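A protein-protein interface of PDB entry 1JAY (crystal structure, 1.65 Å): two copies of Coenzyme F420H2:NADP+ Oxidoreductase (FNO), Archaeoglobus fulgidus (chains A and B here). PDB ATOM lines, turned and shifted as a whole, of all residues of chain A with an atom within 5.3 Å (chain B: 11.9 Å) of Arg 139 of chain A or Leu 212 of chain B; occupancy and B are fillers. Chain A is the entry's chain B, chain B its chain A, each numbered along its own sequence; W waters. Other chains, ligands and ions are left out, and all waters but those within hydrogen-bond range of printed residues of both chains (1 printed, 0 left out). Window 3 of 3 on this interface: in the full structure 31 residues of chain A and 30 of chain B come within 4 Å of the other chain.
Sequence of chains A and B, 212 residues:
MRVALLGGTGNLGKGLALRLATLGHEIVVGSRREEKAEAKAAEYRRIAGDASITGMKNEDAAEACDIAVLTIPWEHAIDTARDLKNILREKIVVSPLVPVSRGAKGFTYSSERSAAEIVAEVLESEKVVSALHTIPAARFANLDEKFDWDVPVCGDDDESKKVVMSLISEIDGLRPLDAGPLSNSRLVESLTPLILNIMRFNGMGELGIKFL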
ATOM      1  N   ARG A  19     -12.499   3.819 -33.639  1.00  0.00           N
ATOM      2  CA  ARG A  19     -13.849   3.361 -34.027  1.00  0.00           C
ATOM      3  C   ARG A  19     -14.213   3.744 -35.458  1.00  0.00           C
ATOM      4  O   ARG A  19     -14.734   2.921 -36.229  1.00  0.00           O
ATOM      5  CB  ARG A  19     -14.919   3.927 -33.077  1.00  0.00           C
ATOM      6  CG  ARG A  19     -14.713   3.634 -31.582  1.00  0.00           C
ATOM      7  CD  ARG A  19     -15.541   2.470 -31.089  1.00  0.00           C
ATOM      8  NE  ARG A  19     -15.103   2.039 -29.762  1.00  0.00           N
ATOM      9  CZ  ARG A  19     -15.248   0.806 -29.293  1.00  0.00           C
ATOM     10  NH1 ARG A  19     -15.837  -0.123 -30.035  1.00  0.00           N
ATOM     11  NH2 ARG A  19     -14.743   0.485 -28.111  1.00  0.00           N
ATOM     12  N   PRO A 136     -17.653   8.149 -22.303  1.00  0.00           N
ATOM     13  CA  PRO A 136     -16.411   8.118 -21.517  1.00  0.00           C
ATOM     14  C   PRO A 136     -15.232   7.627 -22.372  1.00  0.00           C
ATOM     15  O   PRO A 136     -15.277   6.542 -22.948  1.00  0.00           O
ATOM     16  CB  PRO A 136     -16.752   7.209 -20.331  1.00  0.00           C
ATOM     17  CG  PRO A 136     -17.836   6.327 -20.851  1.00  0.00           C
ATOM     18  CD  PRO A 136     -18.650   7.173 -21.812  1.00  0.00           C
ATOM     19  N   ALA A 137     -14.188   8.447 -22.429  1.00  0.00           N
ATOM     20  CA  ALA A 137     -13.042   8.197 -23.303  1.00  0.00           C
ATOM     21  C   ALA A 137     -12.305   6.867 -23.184  1.00  0.00           C
ATOM     22  O   ALA A 137     -12.051   6.204 -24.193  1.00  0.00           O
ATOM     23  CB  ALA A 137     -12.041   9.345 -23.157  1.00  0.00           C
ATOM     24  N   ALA A 138     -11.955   6.482 -21.963  1.00  0.00           N
ATOM     25  CA  ALA A 138     -11.200   5.238 -21.764  1.00  0.00           C
ATOM     26  C   ALA A 138     -11.995   4.018 -22.186  1.00  0.00           C
ATOM     27  O   ALA A 138     -11.490   3.165 -22.933  1.00  0.00           O
ATOM     28  CB  ALA A 138     -10.759   5.118 -20.325  1.00  0.00           C
ATOM     29  N   ARG A 139     -13.237   3.917 -21.728  1.00  0.00           N
ATOM     30  CA  ARG A 139     -14.050   2.776 -22.130  1.00  0.00           C
ATOM     31  C   ARG A 139     -14.278   2.826 -23.645  1.00  0.00           C
ATOM     32  O   ARG A 139     -14.255   1.803 -24.334  1.00  0.00           O
ATOM     33  CB  ARG A 139     -15.397   2.783 -21.393  1.00  0.00           C
ATOM     34  CG  ARG A 139     -15.285   2.448 -19.885  1.00  0.00           C
ATOM     35  CD  ARG A 139     -16.659   2.438 -19.199  1.00  0.00           C
ATOM     36  NE  ARG A 139     -17.516   1.417 -19.771  1.00  0.00           N
ATOM     37  CZ  ARG A 139     -18.832   1.344 -19.595  1.00  0.00           C
ATOM     38  NH1 ARG A 139     -19.474   2.242 -18.840  1.00  0.00           N
ATOM     39  NH2 ARG A 139     -19.514   0.390 -20.211  1.00  0.00           N
ATOM     40  N   PHE A 140     -14.492   4.024 -24.184  1.00  0.00           N
ATOM     41  CA  PHE A 140     -14.729   4.125 -25.618  1.00  0.00           C
ATOM     42  C   PHE A 140     -13.506   3.683 -26.451  1.00  0.00           C
ATOM     43  O   PHE A 140     -13.652   3.118 -27.541  1.00  0.00           O
ATOM     44  CB  PHE A 140     -15.135   5.581 -25.960  1.00  0.00           C
ATOM     45  CG  PHE A 140     -15.639   5.771 -27.368  1.00  0.00           C
ATOM     46  CD1 PHE A 140     -16.709   5.033 -27.850  1.00  0.00           C
ATOM     47  CD2 PHE A 140     -15.098   6.761 -28.177  1.00  0.00           C
ATOM     48  CE1 PHE A 140     -17.240   5.277 -29.107  1.00  0.00           C
ATOM     49  CE2 PHE A 140     -15.612   7.024 -29.439  1.00  0.00           C
ATOM     50  CZ  PHE A 140     -16.694   6.279 -29.913  1.00  0.00           C
ATOM     51  N   ALA A 141     -12.315   3.928 -25.929  1.00  0.00           N
ATOM     52  CA  ALA A 141     -11.079   3.602 -26.651  1.00  0.00           C
ATOM     53  C   ALA A 141     -10.669   2.141 -26.518  1.00  0.00           C
ATOM     54  O   ALA A 141      -9.787   1.688 -27.244  1.00  0.00           O
ATOM     55  CB  ALA A 141      -9.941   4.496 -26.177  1.00  0.00           C
ATOM     56  N   ASN A 142     -11.292   1.426 -25.586  1.00  0.00           N
ATOM     57  CA  ASN A 142     -10.997   0.000 -25.395  1.00  0.00           C
ATOM     58  C   ASN A 142     -11.805  -0.797 -26.421  1.00  0.00           C
ATOM     59  O   ASN A 142     -13.012  -0.990 -26.285  1.00  0.00           O
ATOM     60  CB  ASN A 142     -11.346  -0.416 -23.973  1.00  0.00           C
ATOM     61  CG  ASN A 142     -11.152  -1.903 -23.756  1.00  0.00           C
ATOM     62  OD1 ASN A 142     -10.481  -2.571 -24.557  1.00  0.00           O
ATOM     63  ND2 ASN A 142     -11.738  -2.431 -22.691  1.00  0.00           N
ATOM     64  N   GLU A 145     -14.101  -3.307 -25.240  1.00  0.00           N
ATOM     65  CA  GLU A 145     -15.172  -2.788 -24.388  1.00  0.00           C
ATOM     66  C   GLU A 145     -16.565  -3.005 -24.949  1.00  0.00           C
ATOM     67  O   GLU A 145     -16.807  -2.766 -26.121  1.00  0.00           O
ATOM     68  CB  GLU A 145     -14.968  -1.281 -24.163  1.00  0.00           C
ATOM     69  CG  GLU A 145     -15.921  -0.638 -23.182  1.00  0.00           C
ATOM     70  CD  GLU A 145     -15.599  -1.005 -21.749  1.00  0.00           C
ATOM     71  OE1 GLU A 145     -14.411  -1.256 -21.455  1.00  0.00           O
ATOM     72  OE2 GLU A 145     -16.519  -1.026 -20.911  1.00  0.00           O
ATOM     73  N   LYS A 146     -17.480  -3.442 -24.088  1.00  0.00           N
ATOM     74  CA  LYS A 146     -18.876  -3.660 -24.466  1.00  0.00           C
ATOM     75  C   LYS A 146     -19.664  -2.493 -23.877  1.00  0.00           C
ATOM     76  O   LYS A 146     -19.486  -2.167 -22.702  1.00  0.00           O
ATOM     77  CB  LYS A 146     -19.409  -4.959 -23.833  1.00  0.00           C
ATOM     78  CG  LYS A 146     -18.526  -6.198 -24.024  1.00  0.00           C
ATOM     79  CD  LYS A 146     -19.158  -7.422 -23.356  1.00  0.00           C
ATOM     80  CE  LYS A 146     -18.250  -8.646 -23.437  1.00  0.00           C
ATOM     81  NZ  LYS A 146     -18.900  -9.863 -22.831  1.00  0.00           N
ATOM     82  N   PHE A 147     -20.520  -1.857 -24.671  1.00  0.00           N
ATOM     83  CA  PHE A 147     -21.316  -0.743 -24.150  1.00  0.00           C
ATOM     84  C   PHE A 147     -22.610  -0.497 -24.929  1.00  0.00           C
ATOM     85  O   PHE A 147     -22.745  -0.903 -26.079  1.00  0.00           O
ATOM     86  CB  PHE A 147     -20.469   0.558 -24.077  1.00  0.00           C
ATOM     87  CG  PHE A 147     -19.885   0.992 -25.402  1.00  0.00           C
ATOM     88  CD1 PHE A 147     -18.534   0.814 -25.664  1.00  0.00           C
ATOM     89  CD2 PHE A 147     -20.689   1.556 -26.388  1.00  0.00           C
ATOM     90  CE1 PHE A 147     -17.985   1.181 -26.889  1.00  0.00           C
ATOM     91  CE2 PHE A 147     -20.159   1.929 -27.620  1.00  0.00           C
ATOM     92  CZ  PHE A 147     -18.803   1.741 -27.877  1.00  0.00           C
ATOM     93  N   ASP A 148     -23.561   0.183 -24.289  1.00  0.00           N
ATOM     94  CA  ASP A 148     -24.859   0.475 -24.911  1.00  0.00           C
ATOM     95  C   ASP A 148     -25.226   1.890 -24.462  1.00  0.00           C
ATOM     96  O   ASP A 148     -25.853   2.081 -23.426  1.00  0.00           O
ATOM     97  CB  ASP A 148     -25.903  -0.539 -24.413  1.00  0.00           C
ATOM     98  CG  ASP A 148     -27.276  -0.308 -25.004  1.00  0.00           C
ATOM     99  OD1 ASP A 148     -28.243  -0.970 -24.550  1.00  0.00           O
ATOM    100  OD2 ASP A 148     -27.412   0.537 -25.920  1.00  0.00           O
ATOM    101  N   TRP A 149     -24.829   2.879 -25.252  1.00  0.00           N
ATOM    102  CA  TRP A 149     -25.053   4.268 -24.866  1.00  0.00           C
ATOM    103  C   TRP A 149     -25.849   5.062 -25.872  1.00  0.00           C
ATOM    104  O   TRP A 149     -25.801   4.797 -27.081  1.00  0.00           O
ATOM    105  CB  TRP A 149     -23.707   4.997 -24.687  1.00  0.00           C
ATOM    106  CG  TRP A 149     -22.740   4.419 -23.662  1.00  0.00           C
ATOM    107  CD1 TRP A 149     -23.033   3.954 -22.400  1.00  0.00           C
ATOM    108  CD2 TRP A 149     -21.311   4.340 -23.792  1.00  0.00           C
ATOM    109  NE1 TRP A 149     -21.870   3.596 -21.741  1.00  0.00           N
ATOM    110  CE2 TRP A 149     -20.802   3.823 -22.571  1.00  0.00           C
ATOM    111  CE3 TRP A 149     -20.411   4.654 -24.819  1.00  0.00           C
ATOM    112  CZ2 TRP A 149     -19.426   3.617 -22.358  1.00  0.00           C
ATOM    113  CZ3 TRP A 149     -19.043   4.447 -24.606  1.00  0.00           C
ATOM    114  CH2 TRP A 149     -18.570   3.934 -23.384  1.00  0.00           C
ATOM    115  N   GLU A 206     -16.320   4.930 -15.066  1.00  0.00           N
ATOM    116  CA  GLU A 206     -16.855   5.686 -16.203  1.00  0.00           C
ATOM    117  C   GLU A 206     -18.240   5.235 -16.613  1.00  0.00           C
ATOM    118  O   GLU A 206     -18.511   4.042 -16.771  1.00  0.00           O
ATOM    119  CB  GLU A 206     -15.920   5.589 -17.420  1.00  0.00           C
ATOM    120  CG  GLU A 206     -14.583   6.333 -17.307  1.00  0.00           C
ATOM    121  CD  GLU A 206     -13.827   6.318 -18.642  1.00  0.00           C
ATOM    122  OE1 GLU A 206     -13.909   5.288 -19.329  1.00  0.00           O
ATOM    123  OE2 GLU A 206     -13.151   7.325 -19.028  1.00  0.00           O
ATOM    124  N   LEU A 207     -19.122   6.206 -16.813  1.00  0.00           N
ATOM    125  CA  LEU A 207     -20.492   5.917 -17.184  1.00  0.00           C
ATOM    126  C   LEU A 207     -20.970   6.699 -18.394  1.00  0.00           C
ATOM    127  O   LEU A 207     -20.523   7.823 -18.644  1.00  0.00           O
ATOM    128  CB  LEU A 207     -21.426   6.268 -16.011  1.00  0.00           C
ATOM    129  CG  LEU A 207     -21.206   5.559 -14.680  1.00  0.00           C
ATOM    130  CD1 LEU A 207     -22.008   6.228 -13.560  1.00  0.00           C
ATOM    131  CD2 LEU A 207     -21.598   4.090 -14.834  1.00  0.00           C
ATOM    132  N   GLY A 208     -21.895   6.079 -19.125  1.00  0.00           N
ATOM    133  CA  GLY A 208     -22.554   6.721 -20.241  1.00  0.00           C
ATOM    134  C   GLY A 208     -24.030   6.739 -19.796  1.00  0.00           C
ATOM    135  O   GLY A 208     -24.345   6.376 -18.646  1.00  0.00           O
ATOM    136  N   ILE A 209     -24.936   7.140 -20.688  1.00  0.00           N
ATOM    137  CA  ILE A 209     -26.359   7.178 -20.358  1.00  0.00           C
ATOM    138  C   ILE A 209     -27.231   6.505 -21.396  1.00  0.00           C
ATOM    139  O   ILE A 209     -26.840   6.348 -22.563  1.00  0.00           O
ATOM    140  CB  ILE A 209     -26.849   8.633 -20.171  1.00  0.00           C
ATOM    141  CG1 ILE A 209     -26.354   9.519 -21.312  1.00  0.00           C
ATOM    142  CG2 ILE A 209     -26.268   9.192 -18.886  1.00  0.00           C
ATOM    143  CD1 ILE A 209     -27.362   9.881 -22.316  1.00  0.00           C
ATOM    144  N   LYS A 210     -28.407   6.083 -20.947  1.00  0.00           N
ATOM    145  CA  LYS A 210     -29.381   5.446 -21.820  1.00  0.00           C
ATOM    146  C   LYS A 210     -30.763   5.984 -21.443  1.00  0.00           C
ATOM    147  O   LYS A 210     -31.063   6.141 -20.251  1.00  0.00           O
ATOM    148  CB  LYS A 210     -29.363   3.922 -21.608  1.00  0.00           C
ATOM    149  CG  LYS A 210     -30.156   3.159 -22.629  1.00  0.00           C
ATOM    150  CD  LYS A 210     -29.386   3.107 -23.936  1.00  0.00           C
ATOM    151  CE  LYS A 210     -30.155   2.319 -24.983  1.00  0.00           C
ATOM    152  NZ  LYS A 210     -29.638   2.593 -26.342  1.00  0.00           N
ATOM    153  N   ASP B 148     -36.485   0.045 -15.696  1.00  0.00           N
ATOM    154  CA  ASP B 148     -35.161  -0.066 -15.101  1.00  0.00           C
ATOM    155  C   ASP B 148     -34.616   1.353 -15.149  1.00  0.00           C
ATOM    156  O   ASP B 148     -33.991   1.750 -16.132  1.00  0.00           O
ATOM    157  CB  ASP B 148     -34.270  -0.986 -15.943  1.00  0.00           C
ATOM    158  CG  ASP B 148     -32.908  -1.189 -15.321  1.00  0.00           C
ATOM    159  OD1 ASP B 148     -32.045  -1.831 -15.961  1.00  0.00           O
ATOM    160  OD2 ASP B 148     -32.698  -0.711 -14.187  1.00  0.00           O
ATOM    161  N   TRP B 149     -34.871   2.115 -14.087  1.00  0.00           N
ATOM    162  CA  TRP B 149     -34.443   3.503 -14.039  1.00  0.00           C
ATOM    163  C   TRP B 149     -33.524   3.835 -12.877  1.00  0.00           C
ATOM    164  O   TRP B 149     -33.585   3.205 -11.809  1.00  0.00           O
ATOM    165  CB  TRP B 149     -35.659   4.430 -13.921  1.00  0.00           C
ATOM    166  CG  TRP B 149     -36.635   4.358 -15.039  1.00  0.00           C
ATOM    167  CD1 TRP B 149     -36.357   4.211 -16.368  1.00  0.00           C
ATOM    168  CD2 TRP B 149     -38.050   4.476 -14.931  1.00  0.00           C
ATOM    169  NE1 TRP B 149     -37.523   4.231 -17.100  1.00  0.00           N
ATOM    170  CE2 TRP B 149     -38.578   4.395 -16.237  1.00  0.00           C
ATOM    171  CE3 TRP B 149     -38.930   4.648 -13.850  1.00  0.00           C
ATOM    172  CZ2 TRP B 149     -39.955   4.480 -16.496  1.00  0.00           C
ATOM    173  CZ3 TRP B 149     -40.306   4.732 -14.108  1.00  0.00           C
ATOM    174  CH2 TRP B 149     -40.799   4.648 -15.417  1.00  0.00           C
ATOM    175  N   ASP B 150     -32.666   4.836 -13.100  1.00  0.00           N
ATOM    176  CA  ASP B 150     -31.787   5.339 -12.063  1.00  0.00           C
ATOM    177  C   ASP B 150     -32.419   6.639 -11.559  1.00  0.00           C
ATOM    178  O   ASP B 150     -33.103   7.336 -12.310  1.00  0.00           O
ATOM    179  CB  ASP B 150     -30.379   5.604 -12.625  1.00  0.00           C
ATOM    180  CG  ASP B 150     -29.583   4.327 -12.762  1.00  0.00           C
ATOM    181  OD1 ASP B 150     -29.992   3.324 -12.117  1.00  0.00           O
ATOM    182  OD2 ASP B 150     -28.564   4.320 -13.490  1.00  0.00           O
ATOM    183  N   VAL B 151     -32.196   6.938 -10.290  1.00  0.00           N
ATOM    184  CA  VAL B 151     -32.764   8.126  -9.642  1.00  0.00           C
ATOM    185  C   VAL B 151     -31.642   8.893  -8.941  1.00  0.00           C
ATOM    186  O   VAL B 151     -31.224   8.517  -7.853  1.00  0.00           O
ATOM    187  CB  VAL B 151     -33.822   7.718  -8.549  1.00  0.00           C
ATOM    188  CG1 VAL B 151     -34.471   8.973  -7.905  1.00  0.00           C
ATOM    189  CG2 VAL B 151     -34.908   6.815  -9.169  1.00  0.00           C
ATOM    190  N   PRO B 152     -31.117   9.965  -9.570  1.00  0.00           N
ATOM    191  CA  PRO B 152     -30.049  10.753  -8.940  1.00  0.00           C
ATOM    192  C   PRO B 152     -30.662  11.409  -7.708  1.00  0.00           C
ATOM    193  O   PRO B 152     -31.788  11.930  -7.768  1.00  0.00           O
ATOM    194  CB  PRO B 152     -29.702  11.817 -10.001  1.00  0.00           C
ATOM    195  CG  PRO B 152     -30.062  11.139 -11.298  1.00  0.00           C
ATOM    196  CD  PRO B 152     -31.372  10.420 -10.947  1.00  0.00           C
ATOM    197  N   ARG B 175     -33.057   2.487  -8.950  1.00  0.00           N
ATOM    198  CA  ARG B 175     -31.761   2.421  -8.312  1.00  0.00           C
ATOM    199  C   ARG B 175     -31.366   3.854  -8.017  1.00  0.00           C
ATOM    200  O   ARG B 175     -31.164   4.639  -8.945  1.00  0.00           O
ATOM    201  CB  ARG B 175     -30.688   1.797  -9.218  1.00  0.00           C
ATOM    202  CG  ARG B 175     -29.303   1.898  -8.532  1.00  0.00           C
ATOM    203  CD  ARG B 175     -28.163   1.295  -9.338  1.00  0.00           C
ATOM    204  NE  ARG B 175     -27.997   1.925 -10.646  1.00  0.00           N
ATOM    205  CZ  ARG B 175     -26.898   1.792 -11.382  1.00  0.00           C
ATOM    206  NH1 ARG B 175     -25.888   1.060 -10.914  1.00  0.00           N
ATOM    207  NH2 ARG B 175     -26.811   2.355 -12.585  1.00  0.00           N
ATOM    208  N   PRO B 176     -31.267   4.223  -6.729  1.00  0.00           N
ATOM    209  CA  PRO B 176     -30.884   5.608  -6.387  1.00  0.00           C
ATOM    210  C   PRO B 176     -29.365   5.773  -6.518  1.00  0.00           C
ATOM    211  O   PRO B 176     -28.617   4.829  -6.272  1.00  0.00           O
ATOM    212  CB  PRO B 176     -31.351   5.747  -4.940  1.00  0.00           C
ATOM    213  CG  PRO B 176     -31.049   4.346  -4.378  1.00  0.00           C
ATOM    214  CD  PRO B 176     -31.521   3.419  -5.515  1.00  0.00           C
ATOM    215  N   LEU B 177     -28.907   6.953  -6.930  1.00  0.00           N
ATOM    216  CA  LEU B 177     -27.464   7.199  -7.060  1.00  0.00           C
ATOM    217  C   LEU B 177     -27.185   8.546  -6.421  1.00  0.00           C
ATOM    218  O   LEU B 177     -27.850   9.521  -6.733  1.00  0.00           O
ATOM    219  CB  LEU B 177     -27.051   7.251  -8.543  1.00  0.00           C
ATOM    220  CG  LEU B 177     -27.236   5.969  -9.363  1.00  0.00           C
ATOM    221  CD1 LEU B 177     -26.978   6.256 -10.828  1.00  0.00           C
ATOM    222  CD2 LEU B 177     -26.278   4.893  -8.822  1.00  0.00           C
ATOM    223  N   LEU B 191     -32.238  17.330 -15.935  1.00  0.00           N
ATOM    224  CA  LEU B 191     -32.405  16.108 -16.712  1.00  0.00           C
ATOM    225  C   LEU B 191     -33.793  16.036 -17.306  1.00  0.00           C
ATOM    226  O   LEU B 191     -33.971  15.500 -18.393  1.00  0.00           O
ATOM    227  CB  LEU B 191     -32.238  14.862 -15.850  1.00  0.00           C
ATOM    228  CG  LEU B 191     -30.833  14.576 -15.351  1.00  0.00           C
ATOM    229  CD1 LEU B 191     -30.873  13.388 -14.383  1.00  0.00           C
ATOM    230  CD2 LEU B 191     -29.922  14.301 -16.542  1.00  0.00           C
ATOM    231  N   GLY B 208     -37.241   7.331 -18.840  1.00  0.00           N
ATOM    232  CA  GLY B 208     -36.494   7.545 -17.611  1.00  0.00           C
ATOM    233  C   GLY B 208     -35.063   7.450 -18.117  1.00  0.00           C
ATOM    234  O   GLY B 208     -34.844   7.412 -19.338  1.00  0.00           O
ATOM    235  N   ILE B 209     -34.093   7.425 -17.221  1.00  0.00           N
ATOM    236  CA  ILE B 209     -32.704   7.321 -17.642  1.00  0.00           C
ATOM    237  C   ILE B 209     -31.936   6.300 -16.814  1.00  0.00           C
ATOM    238  O   ILE B 209     -32.312   5.990 -15.679  1.00  0.00           O
ATOM    239  CB  ILE B 209     -31.985   8.675 -17.539  1.00  0.00           C
ATOM    240  CG1 ILE B 209     -32.017   9.177 -16.096  1.00  0.00           C
ATOM    241  CG2 ILE B 209     -32.655   9.676 -18.469  1.00  0.00           C
ATOM    242  CD1 ILE B 209     -31.207  10.434 -15.876  1.00  0.00           C
ATOM    243  N   LYS B 210     -30.855   5.770 -17.392  1.00  0.00           N
ATOM    244  CA  LYS B 210     -30.012   4.782 -16.716  1.00  0.00           C
ATOM    245  C   LYS B 210     -28.552   5.148 -16.966  1.00  0.00           C
ATOM    246  O   LYS B 210     -28.213   5.556 -18.083  1.00  0.00           O
ATOM    247  CB  LYS B 210     -30.269   3.388 -17.301  1.00  0.00           C
ATOM    248  CG  LYS B 210     -29.475   2.272 -16.634  1.00  0.00           C
ATOM    249  CD  LYS B 210     -30.188   1.902 -15.338  1.00  0.00           C
ATOM    250  CE  LYS B 210     -29.452   0.857 -14.525  1.00  0.00           C
ATOM    251  NZ  LYS B 210     -30.108   0.725 -13.175  1.00  0.00           N
ATOM    252  N   PHE B 211     -27.694   5.019 -15.945  1.00  0.00           N
ATOM    253  CA  PHE B 211     -26.260   5.301 -16.133  1.00  0.00           C
ATOM    254  C   PHE B 211     -25.611   3.930 -16.235  1.00  0.00           C
ATOM    255  O   PHE B 211     -25.839   3.072 -15.382  1.00  0.00           O
ATOM    256  CB  PHE B 211     -25.709   6.126 -14.971  1.00  0.00           C
ATOM    257  CG  PHE B 211     -26.375   7.486 -14.857  1.00  0.00           C
ATOM    258  CD1 PHE B 211     -27.542   7.650 -14.114  1.00  0.00           C
ATOM    259  CD2 PHE B 211     -25.888   8.571 -15.575  1.00  0.00           C
ATOM    260  CE1 PHE B 211     -28.226   8.889 -14.093  1.00  0.00           C
ATOM    261  CE2 PHE B 211     -26.558   9.809 -15.563  1.00  0.00           C
ATOM    262  CZ  PHE B 211     -27.735   9.964 -14.819  1.00  0.00           C
ATOM    263  N   LEU B 212     -24.818   3.725 -17.281  1.00  0.00           N
ATOM    264  CA  LEU B 212     -24.225   2.423 -17.535  1.00  0.00           C
ATOM    265  C   LEU B 212     -22.917   2.487 -18.358  1.00  0.00           C
ATOM    266  O   LEU B 212     -22.281   1.416 -18.523  1.00  0.00           O
ATOM    267  CB  LEU B 212     -25.254   1.563 -18.293  1.00  0.00           C
ATOM    268  CG  LEU B 212     -25.595   1.913 -19.769  1.00  0.00           C
ATOM    269  CD1 LEU B 212     -26.743   1.033 -20.215  1.00  0.00           C
ATOM    270  CD2 LEU B 212     -26.010   3.403 -19.968  1.00  0.00           C
ATOM    271  OXT LEU B 212     -22.563   3.567 -18.869  1.00  0.00           O
HETATM  272  O   HOH W   1     -22.865   0.010 -21.378  1.00  0.00           O
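Of the 14 printed residues of chain B, 4 touch a printed residue of chain A. Hydrophobic or aromatic side chains of chain B that line the printed part of chain A: Ile 209, Phe 211 and Leu 212. Of the 18 printed residues of chain A, 7 touch a printed residue of chain B. Along chain A the printed residues that touch a printed residue of chain B span positions 139 to 210. Among the printed residues, 14 pairs touch across the chains.
Among the printed residues, merely in contact across the chains: Asp 148 of chain A with Leu 212 of chain B (3.5 Å), Leu 207 of chain A with Phe 211 of chain B (3.96 Å), Leu 207 of chain A with Leu 212 of chain B (3.5 Å), Gly 208 of chain A with Lys 210 of chain B (3.99 Å), Gly 208 of chain A with Phe 211 of chain B (3.3 Å), Ile 209 of chain A with Lys 210 of chain B (3.4 Å), Ile 209 of chain A with Phe 211 of chain B (3.4 Å), Ile 209 of chain A with Leu 212 of chain B (3.6 Å), Lys 210 of chain A with Ile 209 of chain B (3.3 Å) and Lys 210 of chain A with Leu 212 of chain B (3.7 Å).
The backbone carbonyl oxygen of Lys 210 of chain A lies within hydrogen-bond range of the backbone NH of Lys 210 of chain B (2.9 Å). The indole nitrogen (NE1) of Trp 149 of chain A lies within hydrogen-bond range of the chain-end carboxylate (OXT) of Leu 212 of chain B. The backbone NH (N) of Gly 208 of chain A sits at hydrogen-bond distance from the chain-end carboxylate (OXT) of Leu 212 of chain B. The guanidinium group (NH1) of Arg 139 of chain A is in salt-bridge range of the chain-end carboxylate (O) of Leu 212 of chain B (2.9 Å).
No residue of chain B comes within 4 Å of Pro 136 of chain A. No residue of chain B comes within 4 Å of Ala 137 of chain A. No residue of chain B comes within 4 Å of Ala 138 of chain A. Of chain B, only Leu 212 comes within 4 Å of Arg 139 of chain A. No residue of chain B comes within 4 Å of Phe 140 of chain A. No residue of chain B comes within 4 Å of Ala 141 of chain A. No residue of chain B comes within 4 Å of Asn 142 of chain A. No residue of chain B comes within 4 Å of Glu 145 of chain A. No residue of chain B comes within 4 Å of Phe 147 of chain A. Printed residues of chain B within 4 Å of Asp 148 of chain A: Leu 212 (3.5 Å). Of the printed residues of chain B, Trp 149 of chain A touches Leu 212. No residue of chain B comes within 4 Å of Glu 206 of chain A. Leu 207 of chain A touches just these residues of chain B: Phe 211 (3.96 Å) and Leu 212 (3.5 Å). Ile 209 of chain A touches just these residues of chain B: Lys 210, Phe 211 and Leu 212. Printed residues of chain B within 4 Å of Lys 210 of chain A: Ile 209, Lys 210 and Leu 212. Printed residues of chain A within 4 Å of Ile 209 of chain B: Lys 210. Leu 212 of chain B touches seven residues of chain A. The nearest residue of chain B that does not touch Arg 139 of chain A is Phe 211 of chain B (6.9 Å). The nearest printed residue of chain A that does not touch Lys 210 of chain B is Asp 148 of chain A (6.8 Å).
Water W1 lies within hydrogen-bond range of N of Asp 148 of chain A (3.0 Å) and O of Leu 212 of chain B (3.2 Å).
Gly 208 of chain A touches Lys 210 of chain B, but with the chains exchanged Lys 210 of chain A does not touch Gly 208 of chain B (4.1 Å). Ile 209 of chain A touches Lys 210 of chain B, and with the chains exchanged Lys 210 of chain A touches Ile 209 of chain B. Lys 210 of chain B touches its own counterpart, Lys 210 of chain A. Positions printed for both chains: 148, 149, 208, 209 and 210. Of the 14 pairs that touch across the chains among the printed residues, 3 have their exchanged pair printed and touching as well.
NE of Arg 139 of chain A is in salt-bridge range of OE2 of Glu 145 of chain A, at 2.9 Å. The guanidinium group (NH2) of Arg 175 of chain B lies within hydrogen-bond range of the backbone carbonyl oxygen (O) of Phe 211 of chain B (3.0 Å). The side-chain carboxylate of Asp 148 of chain A lies within salt-bridge range of the side-chain amino group of Lys 210 of chain A (3.1 Å). NZ of Lys 210 of chain B lies within salt-bridge range of OD1 of Asp 150 of chain B, at 2.8 Å. The backbone NH (N) of Asp 150 of chain B lies within hydrogen-bond range of the backbone carbonyl oxygen (O) of Ile 209 of chain B (2.8 Å). N of Arg 139 of chain A lies within hydrogen-bond range of OE1 of Glu 206 of chain A (2.8 Å).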
